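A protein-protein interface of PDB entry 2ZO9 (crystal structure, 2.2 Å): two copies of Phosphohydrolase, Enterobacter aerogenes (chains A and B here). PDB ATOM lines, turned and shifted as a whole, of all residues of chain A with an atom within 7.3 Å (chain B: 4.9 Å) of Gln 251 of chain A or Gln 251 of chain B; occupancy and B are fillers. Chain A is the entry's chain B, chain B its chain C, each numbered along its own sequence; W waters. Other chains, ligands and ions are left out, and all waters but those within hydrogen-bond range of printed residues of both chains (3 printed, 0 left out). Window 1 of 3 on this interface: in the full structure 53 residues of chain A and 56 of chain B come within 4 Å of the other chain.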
ATOM      1  N   SER A 198      -3.904  18.176 -17.331  1.00  0.00           N
ATOM      2  CA  SER A 198      -4.714  16.996 -17.411  1.00  0.00           C
ATOM      3  C   SER A 198      -5.729  17.092 -16.287  1.00  0.00           C
ATOM      4  O   SER A 198      -5.370  17.509 -15.172  1.00  0.00           O
ATOM      5  CB  SER A 198      -3.829  15.783 -17.134  1.00  0.00           C
ATOM      6  OG  SER A 198      -4.610  14.623 -17.050  1.00  0.00           O
ATOM      7  N   LEU A 199      -6.970  16.717 -16.564  1.00  0.00           N
ATOM      8  CA  LEU A 199      -7.919  16.500 -15.502  1.00  0.00           C
ATOM      9  C   LEU A 199      -7.701  15.133 -14.857  1.00  0.00           C
ATOM     10  O   LEU A 199      -8.076  14.094 -15.395  1.00  0.00           O
ATOM     11  CB  LEU A 199      -9.376  16.656 -15.953  1.00  0.00           C
ATOM     12  CG  LEU A 199     -10.204  17.071 -14.718  1.00  0.00           C
ATOM     13  CD1 LEU A 199     -11.366  17.911 -15.133  1.00  0.00           C
ATOM     14  CD2 LEU A 199     -10.692  15.856 -13.935  1.00  0.00           C
ATOM     15  N   THR A 200      -7.055  15.142 -13.711  1.00  0.00           N
ATOM     16  CA  THR A 200      -6.917  13.914 -12.950  1.00  0.00           C
ATOM     17  C   THR A 200      -7.296  14.193 -11.494  1.00  0.00           C
ATOM     18  O   THR A 200      -6.814  15.163 -10.906  1.00  0.00           O
ATOM     19  CB  THR A 200      -5.569  13.106 -13.206  1.00  0.00           C
ATOM     20  OG1 THR A 200      -4.910  12.769 -11.981  1.00  0.00           O
ATOM     21  CG2 THR A 200      -4.607  13.793 -14.124  1.00  0.00           C
ATOM     22  N   MET A 201      -8.191  13.368 -10.963  1.00  0.00           N
ATOM     23  CA  MET A 201      -8.764  13.547  -9.629  1.00  0.00           C
ATOM     24  C   MET A 201      -8.664  12.296  -8.738  1.00  0.00           C
ATOM     25  O   MET A 201      -8.729  11.155  -9.212  1.00  0.00           O
ATOM     26  CB  MET A 201     -10.234  13.978  -9.746  1.00  0.00           C
ATOM     27  CG  MET A 201     -11.107  12.953 -10.434  1.00  0.00           C
ATOM     28  SD  MET A 201     -12.775  13.545 -10.830  1.00  0.00           S
ATOM     29  CE  MET A 201     -13.485  12.103 -11.615  1.00  0.00           C
ATOM     30  N   PRO A 213      -6.715  20.570 -16.645  1.00  0.00           N
ATOM     31  CA  PRO A 213      -6.152  20.760 -17.993  1.00  0.00           C
ATOM     32  C   PRO A 213      -5.463  22.128 -18.129  1.00  0.00           C
ATOM     33  O   PRO A 213      -5.773  23.074 -17.378  1.00  0.00           O
ATOM     34  CB  PRO A 213      -7.388  20.717 -18.891  1.00  0.00           C
ATOM     35  CG  PRO A 213      -8.393  19.953 -18.131  1.00  0.00           C
ATOM     36  CD  PRO A 213      -8.175  20.375 -16.698  1.00  0.00           C
ATOM     37  N   GLN A 218      -1.833  20.114 -23.734  1.00  0.00           N
ATOM     38  CA  GLN A 218      -2.094  19.138 -22.680  1.00  0.00           C
ATOM     39  C   GLN A 218      -0.933  18.128 -22.552  1.00  0.00           C
ATOM     40  O   GLN A 218      -0.089  17.990 -23.460  1.00  0.00           O
ATOM     41  CB  GLN A 218      -3.430  18.416 -22.957  1.00  0.00           C
ATOM     42  CG  GLN A 218      -4.618  19.336 -23.360  1.00  0.00           C
ATOM     43  CD  GLN A 218      -4.924  20.413 -22.312  1.00  0.00           C
ATOM     44  OE1 GLN A 218      -4.997  20.124 -21.111  1.00  0.00           O
ATOM     45  NE2 GLN A 218      -5.089  21.668 -22.772  1.00  0.00           N
ATOM     46  N   VAL A 219      -0.862  17.443 -21.417  1.00  0.00           N
ATOM     47  CA  VAL A 219       0.006  16.276 -21.311  1.00  0.00           C
ATOM     48  C   VAL A 219      -0.769  14.998 -20.974  1.00  0.00           C
ATOM     49  O   VAL A 219      -1.559  14.952 -20.018  1.00  0.00           O
ATOM     50  CB  VAL A 219       1.426  16.488 -20.595  1.00  0.00           C
ATOM     51  CG1 VAL A 219       1.731  17.948 -20.211  1.00  0.00           C
ATOM     52  CG2 VAL A 219       1.759  15.439 -19.540  1.00  0.00           C
ATOM     53  N   PRO A 220      -0.586  13.968 -21.818  1.00  0.00           N
ATOM     54  CA  PRO A 220      -1.335  12.733 -21.608  1.00  0.00           C
ATOM     55  C   PRO A 220      -0.813  11.991 -20.381  1.00  0.00           C
ATOM     56  O   PRO A 220       0.371  12.076 -20.060  1.00  0.00           O
ATOM     57  CB  PRO A 220      -1.064  11.923 -22.896  1.00  0.00           C
ATOM     58  CG  PRO A 220       0.284  12.442 -23.412  1.00  0.00           C
ATOM     59  CD  PRO A 220       0.319  13.909 -22.993  1.00  0.00           C
ATOM     60  N   TYR A 221      -1.693  11.274 -19.694  1.00  0.00           N
ATOM     61  CA  TYR A 221      -1.285  10.448 -18.572  1.00  0.00           C
ATOM     62  C   TYR A 221      -0.782   9.112 -19.122  1.00  0.00           C
ATOM     63  O   TYR A 221      -1.518   8.414 -19.831  1.00  0.00           O
ATOM     64  CB  TYR A 221      -2.481  10.274 -17.642  1.00  0.00           C
ATOM     65  CG  TYR A 221      -2.306   9.445 -16.396  1.00  0.00           C
ATOM     66  CD1 TYR A 221      -2.505  10.018 -15.137  1.00  0.00           C
ATOM     67  CD2 TYR A 221      -1.994   8.084 -16.470  1.00  0.00           C
ATOM     68  CE1 TYR A 221      -2.401   9.270 -13.987  1.00  0.00           C
ATOM     69  CE2 TYR A 221      -1.875   7.318 -15.323  1.00  0.00           C
ATOM     70  CZ  TYR A 221      -2.090   7.915 -14.087  1.00  0.00           C
ATOM     71  OH  TYR A 221      -1.991   7.151 -12.953  1.00  0.00           O
ATOM     72  N   PRO A 234      -8.170  18.752 -26.684  1.00  0.00           N
ATOM     73  CA  PRO A 234      -9.029  19.907 -26.331  1.00  0.00           C
ATOM     74  C   PRO A 234      -8.761  20.531 -24.959  1.00  0.00           C
ATOM     75  O   PRO A 234      -8.600  19.832 -23.975  1.00  0.00           O
ATOM     76  CB  PRO A 234     -10.451  19.321 -26.410  1.00  0.00           C
ATOM     77  CG  PRO A 234     -10.321  18.276 -27.493  1.00  0.00           C
ATOM     78  CD  PRO A 234      -8.974  17.610 -27.165  1.00  0.00           C
ATOM     79  N   ALA A 235      -8.683  21.855 -24.926  1.00  0.00           N
ATOM     80  CA  ALA A 235      -8.426  22.582 -23.698  1.00  0.00           C
ATOM     81  C   ALA A 235      -9.768  22.880 -22.984  1.00  0.00           C
ATOM     82  O   ALA A 235     -10.864  22.937 -23.593  1.00  0.00           O
ATOM     83  CB  ALA A 235      -7.711  23.870 -24.022  1.00  0.00           C
ATOM     84  N   SER A 236      -9.685  23.082 -21.691  1.00  0.00           N
ATOM     85  CA  SER A 236     -10.874  23.371 -20.938  1.00  0.00           C
ATOM     86  C   SER A 236     -10.468  23.964 -19.634  1.00  0.00           C
ATOM     87  O   SER A 236      -9.289  24.030 -19.281  1.00  0.00           O
ATOM     88  CB  SER A 236     -11.717  22.115 -20.688  1.00  0.00           C
ATOM     89  OG  SER A 236     -10.958  21.156 -20.000  1.00  0.00           O
ATOM     90  N   CYS A 237     -11.464  24.413 -18.909  1.00  0.00           N
ATOM     91  CA  CYS A 237     -11.187  24.893 -17.591  1.00  0.00           C
ATOM     92  C   CYS A 237     -12.219  24.299 -16.640  1.00  0.00           C
ATOM     93  O   CYS A 237     -13.123  23.578 -17.071  1.00  0.00           O
ATOM     94  CB  CYS A 237     -11.181  26.422 -17.602  1.00  0.00           C
ATOM     95  SG  CYS A 237     -12.786  27.170 -17.825  1.00  0.00           S
ATOM     96  N   LEU A 238     -12.066  24.585 -15.356  1.00  0.00           N
ATOM     97  CA  LEU A 238     -13.001  24.111 -14.358  1.00  0.00           C
ATOM     98  C   LEU A 238     -13.793  25.312 -13.860  1.00  0.00           C
ATOM     99  O   LEU A 238     -13.228  26.343 -13.556  1.00  0.00           O
ATOM    100  CB  LEU A 238     -12.231  23.471 -13.210  1.00  0.00           C
ATOM    101  CG  LEU A 238     -12.549  22.061 -12.730  1.00  0.00           C
ATOM    102  CD1 LEU A 238     -12.907  21.089 -13.835  1.00  0.00           C
ATOM    103  CD2 LEU A 238     -11.392  21.544 -11.869  1.00  0.00           C
ATOM    104  N   MET A 239     -15.107  25.193 -13.835  1.00  0.00           N
ATOM    105  CA  MET A 239     -15.908  26.134 -13.071  1.00  0.00           C
ATOM    106  C   MET A 239     -16.179  25.548 -11.688  1.00  0.00           C
ATOM    107  O   MET A 239     -16.524  24.361 -11.567  1.00  0.00           O
ATOM    108  CB  MET A 239     -17.231  26.447 -13.768  1.00  0.00           C
ATOM    109  CG  MET A 239     -17.077  26.920 -15.181  1.00  0.00           C
ATOM    110  SD  MET A 239     -16.259  28.515 -15.376  1.00  0.00           S
ATOM    111  CE  MET A 239     -17.414  29.634 -14.665  1.00  0.00           C
ATOM    112  N   SER A 249     -17.514  21.240  -9.049  1.00  0.00           N
ATOM    113  CA  SER A 249     -16.627  21.639 -10.122  1.00  0.00           C
ATOM    114  C   SER A 249     -17.099  20.989 -11.397  1.00  0.00           C
ATOM    115  O   SER A 249     -17.328  19.776 -11.440  1.00  0.00           O
ATOM    116  CB  SER A 249     -15.212  21.172  -9.836  1.00  0.00           C
ATOM    117  OG  SER A 249     -14.848  21.613  -8.559  1.00  0.00           O
ATOM    118  N   TYR A 250     -17.261  21.792 -12.438  1.00  0.00           N
ATOM    119  CA  TYR A 250     -17.624  21.227 -13.744  1.00  0.00           C
ATOM    120  C   TYR A 250     -16.668  21.715 -14.806  1.00  0.00           C
ATOM    121  O   TYR A 250     -16.166  22.844 -14.743  1.00  0.00           O
ATOM    122  CB  TYR A 250     -19.095  21.505 -14.128  1.00  0.00           C
ATOM    123  CG  TYR A 250     -19.509  22.942 -14.155  1.00  0.00           C
ATOM    124  CD1 TYR A 250     -19.471  23.677 -15.347  1.00  0.00           C
ATOM    125  CD2 TYR A 250     -19.970  23.568 -13.000  1.00  0.00           C
ATOM    126  CE1 TYR A 250     -19.870  25.011 -15.384  1.00  0.00           C
ATOM    127  CE2 TYR A 250     -20.382  24.900 -13.016  1.00  0.00           C
ATOM    128  CZ  TYR A 250     -20.330  25.615 -14.212  1.00  0.00           C
ATOM    129  OH  TYR A 250     -20.735  26.940 -14.218  1.00  0.00           O
ATOM    130  N   GLN A 251     -16.428  20.838 -15.777  1.00  0.00           N
ATOM    131  CA  GLN A 251     -15.507  21.132 -16.855  1.00  0.00           C
ATOM    132  C   GLN A 251     -16.202  22.038 -17.878  1.00  0.00           C
ATOM    133  O   GLN A 251     -17.332  21.797 -18.269  1.00  0.00           O
ATOM    134  CB  GLN A 251     -15.018  19.844 -17.487  1.00  0.00           C
ATOM    135  CG  GLN A 251     -14.090  20.073 -18.647  1.00  0.00           C
ATOM    136  CD  GLN A 251     -13.448  18.796 -19.077  1.00  0.00           C
ATOM    137  OE1 GLN A 251     -14.137  17.879 -19.546  1.00  0.00           O
ATOM    138  NE2 GLN A 251     -12.125  18.706 -18.915  1.00  0.00           N
ATOM    139  N   HIS A 252     -15.538  23.121 -18.256  1.00  0.00           N
ATOM    140  CA  HIS A 252     -16.089  24.039 -19.248  1.00  0.00           C
ATOM    141  C   HIS A 252     -15.126  23.997 -20.423  1.00  0.00           C
ATOM    142  O   HIS A 252     -13.967  24.399 -20.282  1.00  0.00           O
ATOM    143  CB  HIS A 252     -16.169  25.457 -18.683  1.00  0.00           C
ATOM    144  CG  HIS A 252     -16.734  26.441 -19.654  1.00  0.00           C
ATOM    145  ND1 HIS A 252     -15.946  27.167 -20.521  1.00  0.00           N
ATOM    146  CD2 HIS A 252     -18.013  26.783 -19.929  1.00  0.00           C
ATOM    147  CE1 HIS A 252     -16.714  27.901 -21.304  1.00  0.00           C
ATOM    148  NE2 HIS A 252     -17.971  27.687 -20.964  1.00  0.00           N
ATOM    149  N   SER A 253     -15.573  23.468 -21.556  1.00  0.00           N
ATOM    150  CA  SER A 253     -14.714  23.327 -22.719  1.00  0.00           C
ATOM    151  C   SER A 253     -14.378  24.705 -23.291  1.00  0.00           C
ATOM    152  O   SER A 253     -15.266  25.577 -23.443  1.00  0.00           O
ATOM    153  CB  SER A 253     -15.402  22.487 -23.797  1.00  0.00           C
ATOM    154  OG  SER A 253     -14.706  22.555 -25.037  1.00  0.00           O
ATOM    155  N   LEU A 254     -13.107  24.890 -23.615  1.00  0.00           N
ATOM    156  CA  LEU A 254     -12.647  26.116 -24.264  1.00  0.00           C
ATOM    157  C   LEU A 254     -12.426  25.963 -25.779  1.00  0.00           C
ATOM    158  O   LEU A 254     -11.882  26.856 -26.421  1.00  0.00           O
ATOM    159  CB  LEU A 254     -11.366  26.621 -23.582  1.00  0.00           C
ATOM    160  CG  LEU A 254     -11.562  26.993 -22.114  1.00  0.00           C
ATOM    161  CD1 LEU A 254     -10.212  27.088 -21.327  1.00  0.00           C
ATOM    162  CD2 LEU A 254     -12.407  28.270 -21.977  1.00  0.00           C
ATOM    163  N   LEU B 199     -18.362  16.275 -17.311  1.00  0.00           N
ATOM    164  CA  LEU B 199     -17.530  15.977 -16.154  1.00  0.00           C
ATOM    165  C   LEU B 199     -17.847  17.003 -15.043  1.00  0.00           C
ATOM    166  O   LEU B 199     -17.519  18.181 -15.112  1.00  0.00           O
ATOM    167  CB  LEU B 199     -16.032  15.935 -16.504  1.00  0.00           C
ATOM    168  CG  LEU B 199     -15.183  15.098 -15.523  1.00  0.00           C
ATOM    169  CD1 LEU B 199     -13.818  14.920 -16.098  1.00  0.00           C
ATOM    170  CD2 LEU B 199     -15.028  15.810 -14.202  1.00  0.00           C
ATOM    171  N   PRO B 213     -18.529  12.751 -18.964  1.00  0.00           N
ATOM    172  CA  PRO B 213     -18.902  13.149 -20.336  1.00  0.00           C
ATOM    173  C   PRO B 213     -19.533  11.969 -21.104  1.00  0.00           C
ATOM    174  O   PRO B 213     -19.293  10.790 -20.759  1.00  0.00           O
ATOM    175  CB  PRO B 213     -17.560  13.503 -20.971  1.00  0.00           C
ATOM    176  CG  PRO B 213     -16.701  13.898 -19.818  1.00  0.00           C
ATOM    177  CD  PRO B 213     -17.092  12.963 -18.708  1.00  0.00           C
ATOM    178  N   SER B 236     -14.973  12.497 -24.186  1.00  0.00           N
ATOM    179  CA  SER B 236     -13.894  11.822 -23.494  1.00  0.00           C
ATOM    180  C   SER B 236     -14.428  10.698 -22.664  1.00  0.00           C
ATOM    181  O   SER B 236     -15.652  10.473 -22.578  1.00  0.00           O
ATOM    182  CB  SER B 236     -13.099  12.785 -22.589  1.00  0.00           C
ATOM    183  OG  SER B 236     -13.926  13.360 -21.620  1.00  0.00           O
ATOM    184  N   CYS B 237     -13.497   9.985 -22.047  1.00  0.00           N
ATOM    185  CA  CYS B 237     -13.876   9.022 -21.067  1.00  0.00           C
ATOM    186  C   CYS B 237     -13.001   9.221 -19.838  1.00  0.00           C
ATOM    187  O   CYS B 237     -12.130  10.098 -19.816  1.00  0.00           O
ATOM    188  CB  CYS B 237     -13.801   7.614 -21.648  1.00  0.00           C
ATOM    189  SG  CYS B 237     -12.151   7.042 -21.952  1.00  0.00           S
ATOM    190  N   LEU B 238     -13.281   8.440 -18.803  1.00  0.00           N
ATOM    191  CA  LEU B 238     -12.489   8.452 -17.583  1.00  0.00           C
ATOM    192  C   LEU B 238     -11.750   7.136 -17.523  1.00  0.00           C
ATOM    193  O   LEU B 238     -12.331   6.087 -17.755  1.00  0.00           O
ATOM    194  CB  LEU B 238     -13.419   8.586 -16.371  1.00  0.00           C
ATOM    195  CG  LEU B 238     -13.182   9.702 -15.356  1.00  0.00           C
ATOM    196  CD1 LEU B 238     -12.743  11.019 -15.998  1.00  0.00           C
ATOM    197  CD2 LEU B 238     -14.382   9.888 -14.395  1.00  0.00           C
ATOM    198  N   SER B 249      -8.592   8.857 -11.075  1.00  0.00           N
ATOM    199  CA  SER B 249      -9.396   8.975 -12.289  1.00  0.00           C
ATOM    200  C   SER B 249      -8.771  10.054 -13.167  1.00  0.00           C
ATOM    201  O   SER B 249      -8.514  11.166 -12.716  1.00  0.00           O
ATOM    202  CB  SER B 249     -10.845   9.346 -11.957  1.00  0.00           C
ATOM    203  OG  SER B 249     -11.480   8.326 -11.218  1.00  0.00           O
ATOM    204  N   TYR B 250      -8.486   9.715 -14.416  1.00  0.00           N
ATOM    205  CA  TYR B 250      -7.984  10.725 -15.342  1.00  0.00           C
ATOM    206  C   TYR B 250      -8.803  10.756 -16.622  1.00  0.00           C
ATOM    207  O   TYR B 250      -9.320   9.746 -17.074  1.00  0.00           O
ATOM    208  CB  TYR B 250      -6.473  10.601 -15.608  1.00  0.00           C
ATOM    209  CG  TYR B 250      -6.000   9.286 -16.165  1.00  0.00           C
ATOM    210  CD1 TYR B 250      -5.863   9.109 -17.548  1.00  0.00           C
ATOM    211  CD2 TYR B 250      -5.682   8.221 -15.315  1.00  0.00           C
ATOM    212  CE1 TYR B 250      -5.398   7.919 -18.087  1.00  0.00           C
ATOM    213  CE2 TYR B 250      -5.227   7.005 -15.833  1.00  0.00           C
ATOM    214  CZ  TYR B 250      -5.097   6.871 -17.225  1.00  0.00           C
ATOM    215  OH  TYR B 250      -4.660   5.683 -17.750  1.00  0.00           O
ATOM    216  N   GLN B 251      -8.939  11.946 -17.176  1.00  0.00           N
ATOM    217  CA  GLN B 251      -9.702  12.129 -18.391  1.00  0.00           C
ATOM    218  C   GLN B 251      -8.899  11.676 -19.619  1.00  0.00           C
ATOM    219  O   GLN B 251      -7.765  12.042 -19.788  1.00  0.00           O
ATOM    220  CB  GLN B 251     -10.149  13.570 -18.505  1.00  0.00           C
ATOM    221  CG  GLN B 251     -10.975  13.835 -19.762  1.00  0.00           C
ATOM    222  CD  GLN B 251     -11.614  15.196 -19.728  1.00  0.00           C
ATOM    223  OE1 GLN B 251     -10.926  16.204 -19.579  1.00  0.00           O
ATOM    224  NE2 GLN B 251     -12.930  15.235 -19.834  1.00  0.00           N
ATOM    225  N   HIS B 252      -9.482  10.814 -20.443  1.00  0.00           N
ATOM    226  CA  HIS B 252      -8.808  10.379 -21.673  1.00  0.00           C
ATOM    227  C   HIS B 252      -9.631  10.910 -22.845  1.00  0.00           C
ATOM    228  O   HIS B 252     -10.795  10.513 -23.023  1.00  0.00           O
ATOM    229  CB  HIS B 252      -8.726   8.866 -21.722  1.00  0.00           C
ATOM    230  CG  HIS B 252      -8.029   8.350 -22.927  1.00  0.00           C
ATOM    231  ND1 HIS B 252      -8.702   8.003 -24.084  1.00  0.00           N
ATOM    232  CD2 HIS B 252      -6.719   8.142 -23.173  1.00  0.00           C
ATOM    233  CE1 HIS B 252      -7.828   7.632 -25.001  1.00  0.00           C
ATOM    234  NE2 HIS B 252      -6.622   7.694 -24.468  1.00  0.00           N
ATOM    235  N   SER B 253      -9.047  11.844 -23.603  1.00  0.00           N
ATOM    236  CA  SER B 253      -9.741  12.479 -24.730  1.00  0.00           C
ATOM    237  C   SER B 253     -10.074  11.454 -25.819  1.00  0.00           C
ATOM    238  O   SER B 253      -9.214  10.631 -26.178  1.00  0.00           O
ATOM    239  CB  SER B 253      -8.872  13.573 -25.351  1.00  0.00           C
ATOM    240  OG  SER B 253      -9.530  14.089 -26.507  1.00  0.00           O
HETATM  241  O   HOH W   1     -17.354  17.854 -19.293  1.00  0.00           O
HETATM  242  O   HOH W   2     -11.051   9.287  -8.535  1.00  0.00           O
HETATM  243  O   HOH W   3      -7.645  15.981 -19.198  1.00  0.00           O
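Hydrophobic or aromatic side chains of chain A that line the printed part of chain B: Leu 199, Met 201, Tyr 221, Pro 234 and Tyr 250.
Of the 10 printed residues of chain B, 6 touch a printed residue of chain A.
Hydrophobic or aromatic side chains of chain B that line the printed part of chain A: Leu 199, Leu 238 and Tyr 250.
The side-chain hydroxyl (OG) of Ser 236 of chain A is in hydrogen-bond range of the side-chain amide nitrogen (NE2) of Gln 251 of chain A, 2.9 Å away.
The backbone carbonyl oxygen (O) of Tyr 250 of chain A sits at hydrogen-bond distance from the backbone NH (N) of Met 239 of chain A, at 2.7 Å.
The side-chain hydroxyl of Ser 236 of chain B is in hydrogen-bond range of the side-chain amide nitrogen of Gln 251 of chain B (2.8 Å).
Of the printed residues of chain B, Thr 200 of chain A touches Ser 249 and Tyr 250.
Pro 220 of chain A touches none of the printed residues of chain B.
Leu 238 of chain A touches none of the printed residues of chain B.
Of the printed residues of chain B, Tyr 250 of chain A touches Leu 199.
Gln 251 of chain A touches just these residues of chain B: Leu 199 (2.9 Å) and Gln 251 (2.9 Å).
Of the printed residues of chain A, Leu 199 of chain B touches Leu 199 (3.9 Å), Tyr 250 (3.3 Å) and Gln 251 (2.9 Å).
Printed residues of chain A within 4 Å of Tyr 250 of chain B: Leu 199, Thr 200 and Tyr 221.
Of chain A, only Leu 199 and Gln 251 come within 4 Å of Gln 251 of chain B.
Printed residues of chain A within 4 Å of Ser 253 of chain B: Pro 234 (3.6 Å).
The backbone carbonyl oxygen (O) of Leu 199 of chain A is in hydrogen-bond range of the backbone NH (N) of Gln 251 of chain B (2.9 Å).
N of Met 201 of chain A is in hydrogen-bond range of O of Ser 249 of chain B (2.8 Å).
The backbone carbonyl oxygen (O) of Leu 199 of chain B sits at hydrogen-bond distance from the backbone NH (N) of Gln 251 of chain A (2.9 Å).
The side-chain amide oxygen (OE1) of Gln 251 of chain B lies within hydrogen-bond range of the side-chain amide nitrogen (NE2) of Gln 251 of chain A (2.9 Å).
Among the printed residues, pairs that only touch across the chains: Thr 200 of chain A with Ser 249 of chain B, Tyr 250 of chain A with Leu 199 of chain B, Leu 199 of chain A with Tyr 250 of chain B, Tyr 221 of chain A with Tyr 250 of chain B, Thr 200 of chain A with Tyr 250 of chain B, Pro 234 of chain A with Ser 253 of chain B, Met 201 of chain A with Leu 238 of chain B, Leu 199 of chain A with Leu 199 of chain B and Leu 199 of chain A with Ser 249 of chain B.
Leu 199 of chain A touches its own counterpart, Leu 199 of chain B.
Leu 199 of chain A touches Ser 249 of chain B, but with the chains exchanged Ser 249 of chain A does not touch Leu 199 of chain B (4.01 Å).
Leu 199 of chain A touches Tyr 250 of chain B, and with the chains exchanged Tyr 250 of chain A touches Leu 199 of chain B.
Leu 199 of chain A touches Gln 251 of chain B, and with the chains exchanged Gln 251 of chain A touches Leu 199 of chain B.
Positions printed for both chains: 199, 213, 236, 237, 238, 249, 250, 251, 252 and 253.
Of the 13 pairs that touch across the chains among the printed residues, 6 have their exchanged pair printed and touching as well.
Water W1 lies within hydrogen-bond range of N of Leu 199 of chain B and OE1 of Gln 251 of chain A.
Water W3 lies within hydrogen-bond range of N of Leu 199 of chain A and OE1 of Gln 251 of chain B.
Water W2 bridges OG of Ser 249 of chain B and O of Met 201 of chain A.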
